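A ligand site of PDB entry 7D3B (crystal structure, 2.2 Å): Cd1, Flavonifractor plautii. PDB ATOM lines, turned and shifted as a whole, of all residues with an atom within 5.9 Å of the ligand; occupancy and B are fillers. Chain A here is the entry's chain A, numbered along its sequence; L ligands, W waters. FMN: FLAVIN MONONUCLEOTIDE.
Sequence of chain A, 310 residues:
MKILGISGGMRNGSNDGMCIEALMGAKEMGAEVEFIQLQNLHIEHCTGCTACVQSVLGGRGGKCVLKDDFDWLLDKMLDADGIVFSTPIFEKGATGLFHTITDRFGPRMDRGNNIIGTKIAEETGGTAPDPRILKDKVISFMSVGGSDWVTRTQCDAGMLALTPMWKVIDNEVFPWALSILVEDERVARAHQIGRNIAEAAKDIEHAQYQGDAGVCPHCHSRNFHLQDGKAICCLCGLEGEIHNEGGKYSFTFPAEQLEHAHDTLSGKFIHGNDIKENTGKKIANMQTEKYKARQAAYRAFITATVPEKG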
ATOM      1  N   SER A   7     -16.547  37.975   3.312  1.00  0.00           N
ATOM      2  CA  SER A   7     -16.970  36.781   4.034  1.00  0.00           C
ATOM      3  C   SER A   7     -15.997  35.638   3.798  1.00  0.00           C
ATOM      4  O   SER A   7     -15.545  35.421   2.672  1.00  0.00           O
ATOM      5  CB  SER A   7     -18.362  36.330   3.612  1.00  0.00           C
ATOM      6  OG  SER A   7     -18.615  35.024   4.120  1.00  0.00           O
ATOM      7  N   GLY A   8     -15.697  34.902   4.875  1.00  0.00           N
ATOM      8  CA  GLY A   8     -14.846  33.739   4.769  1.00  0.00           C
ATOM      9  C   GLY A   8     -15.573  32.425   4.993  1.00  0.00           C
ATOM     10  O   GLY A   8     -14.934  31.415   5.286  1.00  0.00           O
ATOM     11  N   GLY A   9     -16.899  32.428   4.864  1.00  0.00           N
ATOM     12  CA  GLY A   9     -17.682  31.219   4.995  1.00  0.00           C
ATOM     13  C   GLY A   9     -17.836  30.493   3.667  1.00  0.00           C
ATOM     14  O   GLY A   9     -17.174  30.785   2.668  1.00  0.00           O
ATOM     15  N   MET A  10     -18.739  29.509   3.666  1.00  0.00           N
ATOM     16  CA  MET A  10     -19.146  28.825   2.436  1.00  0.00           C
ATOM     17  C   MET A  10     -19.971  29.759   1.553  1.00  0.00           C
ATOM     18  O   MET A  10     -20.678  30.628   2.078  1.00  0.00           O
ATOM     19  CB  MET A  10     -19.964  27.550   2.736  1.00  0.00           C
ATOM     20  CG  MET A  10     -19.191  26.308   3.216  1.00  0.00           C
ATOM     21  SD  MET A  10     -17.533  25.759   2.285  1.00  0.00           S
ATOM     22  CE  MET A  10     -17.966  26.324   0.449  1.00  0.00           C
ATOM     23  N   GLY A  13     -23.500  30.864   2.556  1.00  0.00           N
ATOM     24  CA  GLY A  13     -23.651  30.438   3.932  1.00  0.00           C
ATOM     25  C   GLY A  13     -24.090  31.565   4.848  1.00  0.00           C
ATOM     26  O   GLY A  13     -24.409  32.674   4.428  1.00  0.00           O
ATOM     27  N   SER A  14     -24.059  31.257   6.155  1.00  0.00           N
ATOM     28  CA  SER A  14     -24.489  32.232   7.157  1.00  0.00           C
ATOM     29  C   SER A  14     -23.592  33.470   7.179  1.00  0.00           C
ATOM     30  O   SER A  14     -24.089  34.600   7.291  1.00  0.00           O
ATOM     31  CB  SER A  14     -24.525  31.566   8.529  1.00  0.00           C
ATOM     32  OG  SER A  14     -25.509  30.549   8.549  1.00  0.00           O
ATOM     33  N   ASN A  15     -22.263  33.282   7.085  1.00  0.00           N
ATOM     34  CA  ASN A  15     -21.355  34.431   7.043  1.00  0.00           C
ATOM     35  C   ASN A  15     -21.630  35.315   5.834  1.00  0.00           C
ATOM     36  O   ASN A  15     -21.524  36.542   5.919  1.00  0.00           O
ATOM     37  CB  ASN A  15     -19.900  33.972   7.043  1.00  0.00           C
ATOM     38  CG  ASN A  15     -19.420  33.602   8.428  1.00  0.00           C
ATOM     39  OD1 ASN A  15     -19.058  34.475   9.219  1.00  0.00           O
ATOM     40  ND2 ASN A  15     -19.391  32.320   8.727  1.00  0.00           N
ATOM     41  N   ASP A  16     -21.960  34.720   4.686  1.00  0.00           N
ATOM     42  CA  ASP A  16     -22.377  35.520   3.533  1.00  0.00           C
ATOM     43  C   ASP A  16     -23.598  36.359   3.887  1.00  0.00           C
ATOM     44  O   ASP A  16     -23.627  37.575   3.620  1.00  0.00           O
ATOM     45  CB  ASP A  16     -22.696  34.619   2.335  1.00  0.00           C
ATOM     46  CG  ASP A  16     -21.441  34.177   1.541  1.00  0.00           C
ATOM     47  OD1 ASP A  16     -20.300  34.294   2.029  1.00  0.00           O
ATOM     48  OD2 ASP A  16     -21.607  33.690   0.398  1.00  0.00           O
ATOM     49  N   PRO A  88     -16.273  32.640   9.742  1.00  0.00           N
ATOM     50  CA  PRO A  88     -16.564  31.457  10.551  1.00  0.00           C
ATOM     51  C   PRO A  88     -15.569  31.321  11.692  1.00  0.00           C
ATOM     52  O   PRO A  88     -14.439  31.793  11.621  1.00  0.00           O
ATOM     53  CB  PRO A  88     -16.399  30.299   9.574  1.00  0.00           C
ATOM     54  CG  PRO A  88     -16.222  30.899   8.244  1.00  0.00           C
ATOM     55  CD  PRO A  88     -15.839  32.306   8.373  1.00  0.00           C
ATOM     56  N   ILE A  89     -16.001  30.615  12.734  1.00  0.00           N
ATOM     57  CA  ILE A  89     -15.155  30.281  13.865  1.00  0.00           C
ATOM     58  C   ILE A  89     -14.689  28.837  13.729  1.00  0.00           C
ATOM     59  O   ILE A  89     -15.513  27.922  13.623  1.00  0.00           O
ATOM     60  CB  ILE A  89     -15.918  30.476  15.188  1.00  0.00           C
ATOM     61  CG1 ILE A  89     -16.280  31.947  15.381  1.00  0.00           C
ATOM     62  CG2 ILE A  89     -15.064  29.967  16.345  1.00  0.00           C
ATOM     63  CD1 ILE A  89     -17.076  32.235  16.675  1.00  0.00           C
ATOM     64  N   PHE A  90     -13.377  28.602  13.734  1.00  0.00           N
ATOM     65  CA  PHE A  90     -12.799  27.265  13.715  1.00  0.00           C
ATOM     66  C   PHE A  90     -11.909  27.087  14.928  1.00  0.00           C
ATOM     67  O   PHE A  90     -11.000  27.897  15.153  1.00  0.00           O
ATOM     68  CB  PHE A  90     -11.947  26.987  12.454  1.00  0.00           C
ATOM     69  CG  PHE A  90     -12.722  26.922  11.142  1.00  0.00           C
ATOM     70  CD1 PHE A  90     -12.036  26.814   9.934  1.00  0.00           C
ATOM     71  CD2 PHE A  90     -14.101  26.984  11.101  1.00  0.00           C
ATOM     72  CE1 PHE A  90     -12.720  26.745   8.708  1.00  0.00           C
ATOM     73  CE2 PHE A  90     -14.795  26.909   9.882  1.00  0.00           C
ATOM     74  CZ  PHE A  90     -14.101  26.792   8.693  1.00  0.00           C
ATOM     75  N   GLU A  91     -12.130  26.015  15.679  1.00  0.00           N
ATOM     76  CA  GLU A  91     -11.388  25.737  16.916  1.00  0.00           C
ATOM     77  C   GLU A  91     -11.235  26.984  17.782  1.00  0.00           C
ATOM     78  O   GLU A  91     -10.144  27.296  18.264  1.00  0.00           O
ATOM     79  CB  GLU A  91     -10.007  25.137  16.643  1.00  0.00           C
ATOM     80  CG  GLU A  91     -10.032  23.911  15.787  1.00  0.00           C
ATOM     81  CD  GLU A  91      -9.800  24.270  14.342  1.00  0.00           C
ATOM     82  OE1 GLU A  91     -10.527  23.723  13.495  1.00  0.00           O
ATOM     83  OE2 GLU A  91      -8.911  25.112  14.063  1.00  0.00           O
ATOM     84  N   LYS A  92     -12.331  27.696  17.979  1.00  0.00           N
ATOM     85  CA  LYS A  92     -12.459  28.824  18.894  1.00  0.00           C
ATOM     86  C   LYS A  92     -11.985  30.140  18.293  1.00  0.00           C
ATOM     87  O   LYS A  92     -12.234  31.190  18.876  1.00  0.00           O
ATOM     88  CB  LYS A  92     -11.709  28.599  20.221  1.00  0.00           C
ATOM     89  CG  LYS A  92     -12.205  27.371  20.988  1.00  0.00           C
ATOM     90  CD  LYS A  92     -11.394  27.110  22.229  1.00  0.00           C
ATOM     91  CE  LYS A  92     -11.798  25.770  22.845  1.00  0.00           C
ATOM     92  NZ  LYS A  92     -11.309  25.584  24.233  1.00  0.00           N
ATOM     93  N   GLY A  93     -11.320  30.127  17.139  1.00  0.00           N
ATOM     94  CA  GLY A  93     -10.813  31.349  16.566  1.00  0.00           C
ATOM     95  C   GLY A  93     -11.256  31.522  15.127  1.00  0.00           C
ATOM     96  O   GLY A  93     -12.168  30.829  14.679  1.00  0.00           O
ATOM     97  N   VAL A 144     -18.827  34.057  13.400  1.00  0.00           N
ATOM     98  CA  VAL A 144     -20.025  33.237  13.438  1.00  0.00           C
ATOM     99  C   VAL A 144     -19.604  31.792  13.635  1.00  0.00           C
ATOM    100  O   VAL A 144     -18.920  31.219  12.793  1.00  0.00           O
ATOM    101  CB  VAL A 144     -20.855  33.396  12.148  1.00  0.00           C
ATOM    102  CG1 VAL A 144     -22.147  32.631  12.292  1.00  0.00           C
ATOM    103  CG2 VAL A 144     -21.130  34.890  11.874  1.00  0.00           C
ATOM    104  N   GLY A 145     -20.012  31.199  14.767  1.00  0.00           N
ATOM    105  CA  GLY A 145     -19.764  29.810  15.054  1.00  0.00           C
ATOM    106  C   GLY A 145     -21.058  29.039  15.310  1.00  0.00           C
ATOM    107  O   GLY A 145     -22.150  29.612  15.345  1.00  0.00           O
ATOM    108  N   GLY A 146     -20.904  27.722  15.493  1.00  0.00           N
ATOM    109  CA  GLY A 146     -22.068  26.876  15.704  1.00  0.00           C
ATOM    110  C   GLY A 146     -22.220  26.375  17.129  1.00  0.00           C
ATOM    111  O   GLY A 146     -23.170  25.653  17.450  1.00  0.00           O
ATOM    112  N   SER A 147     -21.283  26.755  17.987  1.00  0.00           N
ATOM    113  CA  SER A 147     -21.380  26.398  19.395  1.00  0.00           C
ATOM    114  C   SER A 147     -20.909  27.556  20.256  1.00  0.00           C
ATOM    115  O   SER A 147     -21.012  28.713  19.857  1.00  0.00           O
ATOM    116  CB  SER A 147     -20.567  25.137  19.693  1.00  0.00           C
ATOM    117  OG  SER A 147     -19.191  25.441  19.762  1.00  0.00           O
ATOM    118  N   ASP A 148     -20.405  27.270  21.460  1.00  0.00           N
ATOM    119  CA  ASP A 148     -19.877  28.330  22.302  1.00  0.00           C
ATOM    120  C   ASP A 148     -18.354  28.255  22.415  1.00  0.00           C
ATOM    121  O   ASP A 148     -17.777  28.884  23.311  1.00  0.00           O
ATOM    122  CB  ASP A 148     -20.544  28.317  23.684  1.00  0.00           C
ATOM    123  CG  ASP A 148     -20.284  27.039  24.466  1.00  0.00           C
ATOM    124  OD1 ASP A 148     -19.739  26.050  23.917  1.00  0.00           O
ATOM    125  OD2 ASP A 148     -20.651  27.023  25.671  1.00  0.00           O
ATOM    126  N   TRP A 149     -17.707  27.488  21.539  1.00  0.00           N
ATOM    127  CA  TRP A 149     -16.245  27.452  21.450  1.00  0.00           C
ATOM    128  C   TRP A 149     -15.809  28.691  20.673  1.00  0.00           C
ATOM    129  O   TRP A 149     -15.490  28.636  19.481  1.00  0.00           O
ATOM    130  CB  TRP A 149     -15.761  26.175  20.764  1.00  0.00           C
ATOM    131  CG  TRP A 149     -16.026  24.884  21.464  1.00  0.00           C
ATOM    132  CD1 TRP A 149     -17.057  24.591  22.332  1.00  0.00           C
ATOM    133  CD2 TRP A 149     -15.254  23.676  21.361  1.00  0.00           C
ATOM    134  NE1 TRP A 149     -16.961  23.283  22.771  1.00  0.00           N
ATOM    135  CE2 TRP A 149     -15.871  22.702  22.186  1.00  0.00           C
ATOM    136  CE3 TRP A 149     -14.104  23.334  20.653  1.00  0.00           C
ATOM    137  CZ2 TRP A 149     -15.360  21.410  22.316  1.00  0.00           C
ATOM    138  CZ3 TRP A 149     -13.604  22.042  20.783  1.00  0.00           C
ATOM    139  CH2 TRP A 149     -14.222  21.104  21.605  1.00  0.00           C
ATOM    140  N   VAL A 150     -15.820  29.841  21.332  1.00  0.00           N
ATOM    141  CA  VAL A 150     -15.701  31.090  20.596  1.00  0.00           C
ATOM    142  C   VAL A 150     -14.727  32.052  21.274  1.00  0.00           C
ATOM    143  O   VAL A 150     -14.686  33.237  20.936  1.00  0.00           O
ATOM    144  CB  VAL A 150     -17.084  31.736  20.385  1.00  0.00           C
ATOM    145  CG1 VAL A 150     -17.995  30.780  19.587  1.00  0.00           C
ATOM    146  CG2 VAL A 150     -17.746  32.084  21.723  1.00  0.00           C
ATOM    147  N   PRO A 175     -22.255  33.038  18.983  1.00  0.00           N
ATOM    148  CA  PRO A 175     -22.241  31.593  19.220  1.00  0.00           C
ATOM    149  C   PRO A 175     -23.563  30.957  18.811  1.00  0.00           C
ATOM    150  O   PRO A 175     -24.548  31.640  18.535  1.00  0.00           O
ATOM    151  CB  PRO A 175     -22.009  31.470  20.731  1.00  0.00           C
ATOM    152  CG  PRO A 175     -22.514  32.801  21.297  1.00  0.00           C
ATOM    153  CD  PRO A 175     -22.328  33.831  20.229  1.00  0.00           C
ATOM    154  N   TRP A 176     -23.568  29.625  18.788  1.00  0.00           N
ATOM    155  CA  TRP A 176     -24.765  28.846  18.513  1.00  0.00           C
ATOM    156  C   TRP A 176     -25.503  29.393  17.294  1.00  0.00           C
ATOM    157  O   TRP A 176     -26.710  29.644  17.341  1.00  0.00           O
ATOM    158  CB  TRP A 176     -25.687  28.826  19.734  1.00  0.00           C
ATOM    159  CG  TRP A 176     -25.037  28.458  21.028  1.00  0.00           C
ATOM    160  CD1 TRP A 176     -24.770  29.283  22.086  1.00  0.00           C
ATOM    161  CD2 TRP A 176     -24.572  27.159  21.406  1.00  0.00           C
ATOM    162  NE1 TRP A 176     -24.162  28.575  23.097  1.00  0.00           N
ATOM    163  CE2 TRP A 176     -24.030  27.268  22.715  1.00  0.00           C
ATOM    164  CE3 TRP A 176     -24.558  25.904  20.768  1.00  0.00           C
ATOM    165  CZ2 TRP A 176     -23.478  26.176  23.394  1.00  0.00           C
ATOM    166  CZ3 TRP A 176     -24.004  24.817  21.438  1.00  0.00           C
ATOM    167  CH2 TRP A 176     -23.474  24.962  22.744  1.00  0.00           C
ATOM    168  N   ALA A 177     -24.784  29.591  16.186  1.00  0.00           N
ATOM    169  CA  ALA A 177     -25.293  30.366  15.058  1.00  0.00           C
ATOM    170  C   ALA A 177     -25.477  29.564  13.776  1.00  0.00           C
ATOM    171  O   ALA A 177     -25.444  30.128  12.681  1.00  0.00           O
ATOM    172  CB  ALA A 177     -24.395  31.572  14.794  1.00  0.00           C
ATOM    173  N   LEU A 178     -25.686  28.249  13.864  1.00  0.00           N
ATOM    174  CA  LEU A 178     -25.889  27.496  12.633  1.00  0.00           C
ATOM    175  C   LEU A 178     -27.180  27.929  11.945  1.00  0.00           C
ATOM    176  O   LEU A 178     -27.246  27.992  10.713  1.00  0.00           O
ATOM    177  CB  LEU A 178     -25.896  25.994  12.905  1.00  0.00           C
ATOM    178  CG  LEU A 178     -24.570  25.304  13.201  1.00  0.00           C
ATOM    179  CD1 LEU A 178     -24.816  23.803  13.363  1.00  0.00           C
ATOM    180  CD2 LEU A 178     -23.553  25.545  12.117  1.00  0.00           C
HETATM  181  N1  FMN L   1     -17.984  26.744  15.621  1.00  0.00           N
HETATM  182  C2  FMN L   1     -17.661  27.205  16.819  1.00  0.00           C
HETATM  183  O2  FMN L   1     -18.463  27.932  17.370  1.00  0.00           O
HETATM  184  N3  FMN L   1     -16.532  26.919  17.441  1.00  0.00           N
HETATM  185  C4  FMN L   1     -15.628  26.153  16.898  1.00  0.00           C
HETATM  186  O4  FMN L   1     -14.617  25.889  17.478  1.00  0.00           O
HETATM  187  C4A FMN L   1     -15.895  25.593  15.600  1.00  0.00           C
HETATM  188  N5  FMN L   1     -15.007  24.819  15.028  1.00  0.00           N
HETATM  189  C5A FMN L   1     -15.277  24.353  13.808  1.00  0.00           C
HETATM  190  C6  FMN L   1     -14.356  23.541  13.227  1.00  0.00           C
HETATM  191  C7  FMN L   1     -14.599  23.034  11.963  1.00  0.00           C
HETATM  192  C7M FMN L   1     -13.586  22.142  11.319  1.00  0.00           C
HETATM  193  C8  FMN L   1     -15.862  23.353  11.257  1.00  0.00           C
HETATM  194  C8M FMN L   1     -16.142  22.805   9.896  1.00  0.00           C
HETATM  195  C9  FMN L   1     -16.795  24.163  11.859  1.00  0.00           C
HETATM  196  C9A FMN L   1     -16.540  24.667  13.111  1.00  0.00           C
HETATM  197  N10 FMN L   1     -17.474  25.486  13.718  1.00  0.00           N
HETATM  198  C10 FMN L   1     -17.158  25.961  14.970  1.00  0.00           C
HETATM  199  C1' FMN L   1     -18.702  25.823  13.048  1.00  0.00           C
HETATM  200  C2' FMN L   1     -18.466  26.800  11.919  1.00  0.00           C
HETATM  201  O2' FMN L   1     -18.187  28.061  12.443  1.00  0.00           O
HETATM  202  C3' FMN L   1     -19.723  26.976  11.141  1.00  0.00           C
HETATM  203  O3' FMN L   1     -19.874  25.793  10.406  1.00  0.00           O
HETATM  204  C4' FMN L   1     -19.702  28.225  10.282  1.00  0.00           C
HETATM  205  O4' FMN L   1     -20.223  29.289  11.051  1.00  0.00           O
HETATM  206  C5' FMN L   1     -20.557  28.113   9.076  1.00  0.00           C
HETATM  207  O5' FMN L   1     -20.626  29.336   8.428  1.00  0.00           O
HETATM  208  P   FMN L   1     -21.008  29.409   6.934  1.00  0.00           P
HETATM  209  O1P FMN L   1     -20.770  30.721   6.476  1.00  0.00           O
HETATM  210  O2P FMN L   1     -20.191  28.415   6.286  1.00  0.00           O
HETATM  211  O3P FMN L   1     -22.428  29.090   7.005  1.00  0.00           O
HETATM  212  O   HOH W   1     -24.186  28.043   8.958  1.00  0.00           O
HETATM  213  O   HOH W   2     -18.074  25.593   8.412  1.00  0.00           O
HETATM  214  O   HOH W   3     -23.090  29.174  11.564  1.00  0.00           O
HETATM  215  O   HOH W   4     -17.678  27.840   6.922  1.00  0.00           O
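N of Ser 14 sits at hydrogen-bond distance from O3P of the ligand, at 2.8 Å. The backbone carbonyl oxygen (O) of Trp 149 lies within hydrogen-bond range of a nitrogen (N3) of the ligand (2.9 Å). O2' of the ligand lies within hydrogen-bond range of N of Ile 89, at 3.4 Å. O of Ile 89 lies close to O2' of the ligand (2.9 Å). The backbone carbonyl oxygen of Val 144 lies within hydrogen-bond range of an oxygen (O4') of the ligand (2.9 Å). An oxygen (O4) of the ligand sits at hydrogen-bond distance from the backbone NH (N) of Lys 92 (3.0 Å). The backbone NH (N) of Asn 15 is in hydrogen-bond range of an oxygen (O1P) of the ligand (3.0 Å). An oxygen (O1P) of the ligand is in hydrogen-bond range of the side-chain amide nitrogen of Asn 15, 3.1 Å away. N of Glu 91 lies within hydrogen-bond range of O4 of the ligand (3.1 Å). The backbone NH (N) of Gly 146 lies within hydrogen-bond range of a nitrogen (N1) of the ligand (3.1 Å). The backbone NH of Ser 147 is in hydrogen-bond range of an oxygen (O2) of the ligand, 3.1 Å away. The backbone NH of Met 10 is in hydrogen-bond range of an oxygen (O2P) of the ligand (3.2 Å).
The side-chain hydroxyl (OG) of Ser 147 is in hydrogen-bond range of the backbone NH (N) of Trp 149 (3.1 Å). The backbone NH (N) of Ile 89 lies within hydrogen-bond range of the backbone carbonyl oxygen (O) of Val 144 (3.0 Å). O of Ser 147 is in hydrogen-bond range of N of Trp 176 (2.9 Å). O of Gly 145 is in hydrogen-bond range of N of Ala 177. The backbone NH (N) of Gly 9 lies within hydrogen-bond range of the side-chain hydroxyl (OG) of Ser 7, 3.2 Å away.
CA of Gly 9 touches O1P of the ligand (3.5 Å). Gly 13 touches the ligand (CA to O3P, 3.6 Å). Pro 88 touches the ligand (CB to C4', 3.96 Å). CA of Phe 90 touches N5 of the ligand (3.5 Å). Gly 145 touches the ligand (CA to O2, 3.3 Å). Val 150 touches the ligand (CG1 to O2, 3.6 Å). Hydrophobic or aromatic side chains that line the ligand: Met 10, Pro 88, Ile 89, Phe 90, Trp 149 and Val 150. 16 residues have an atom within 4 Å of the ligand: Gly 9, Met 10, Gly 13, Ser 14, Asn 15, Pro 88, Ile 89, Phe 90, Glu 91, Lys 92, Val 144, Gly 145, Gly 146, Ser 147, Trp 149 and Val 150. The nearest printed residue that does not touch the ligand is Leu 178 (4.1 Å).
Water W1 lies within hydrogen-bond range of an oxygen (O3P) of the ligand (2.8 Å) and the side-chain hydroxyl (OG) of Ser 14 (2.9 Å). Water W3 lies within hydrogen-bond range of O of Ala 177 and O4' of the ligand.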
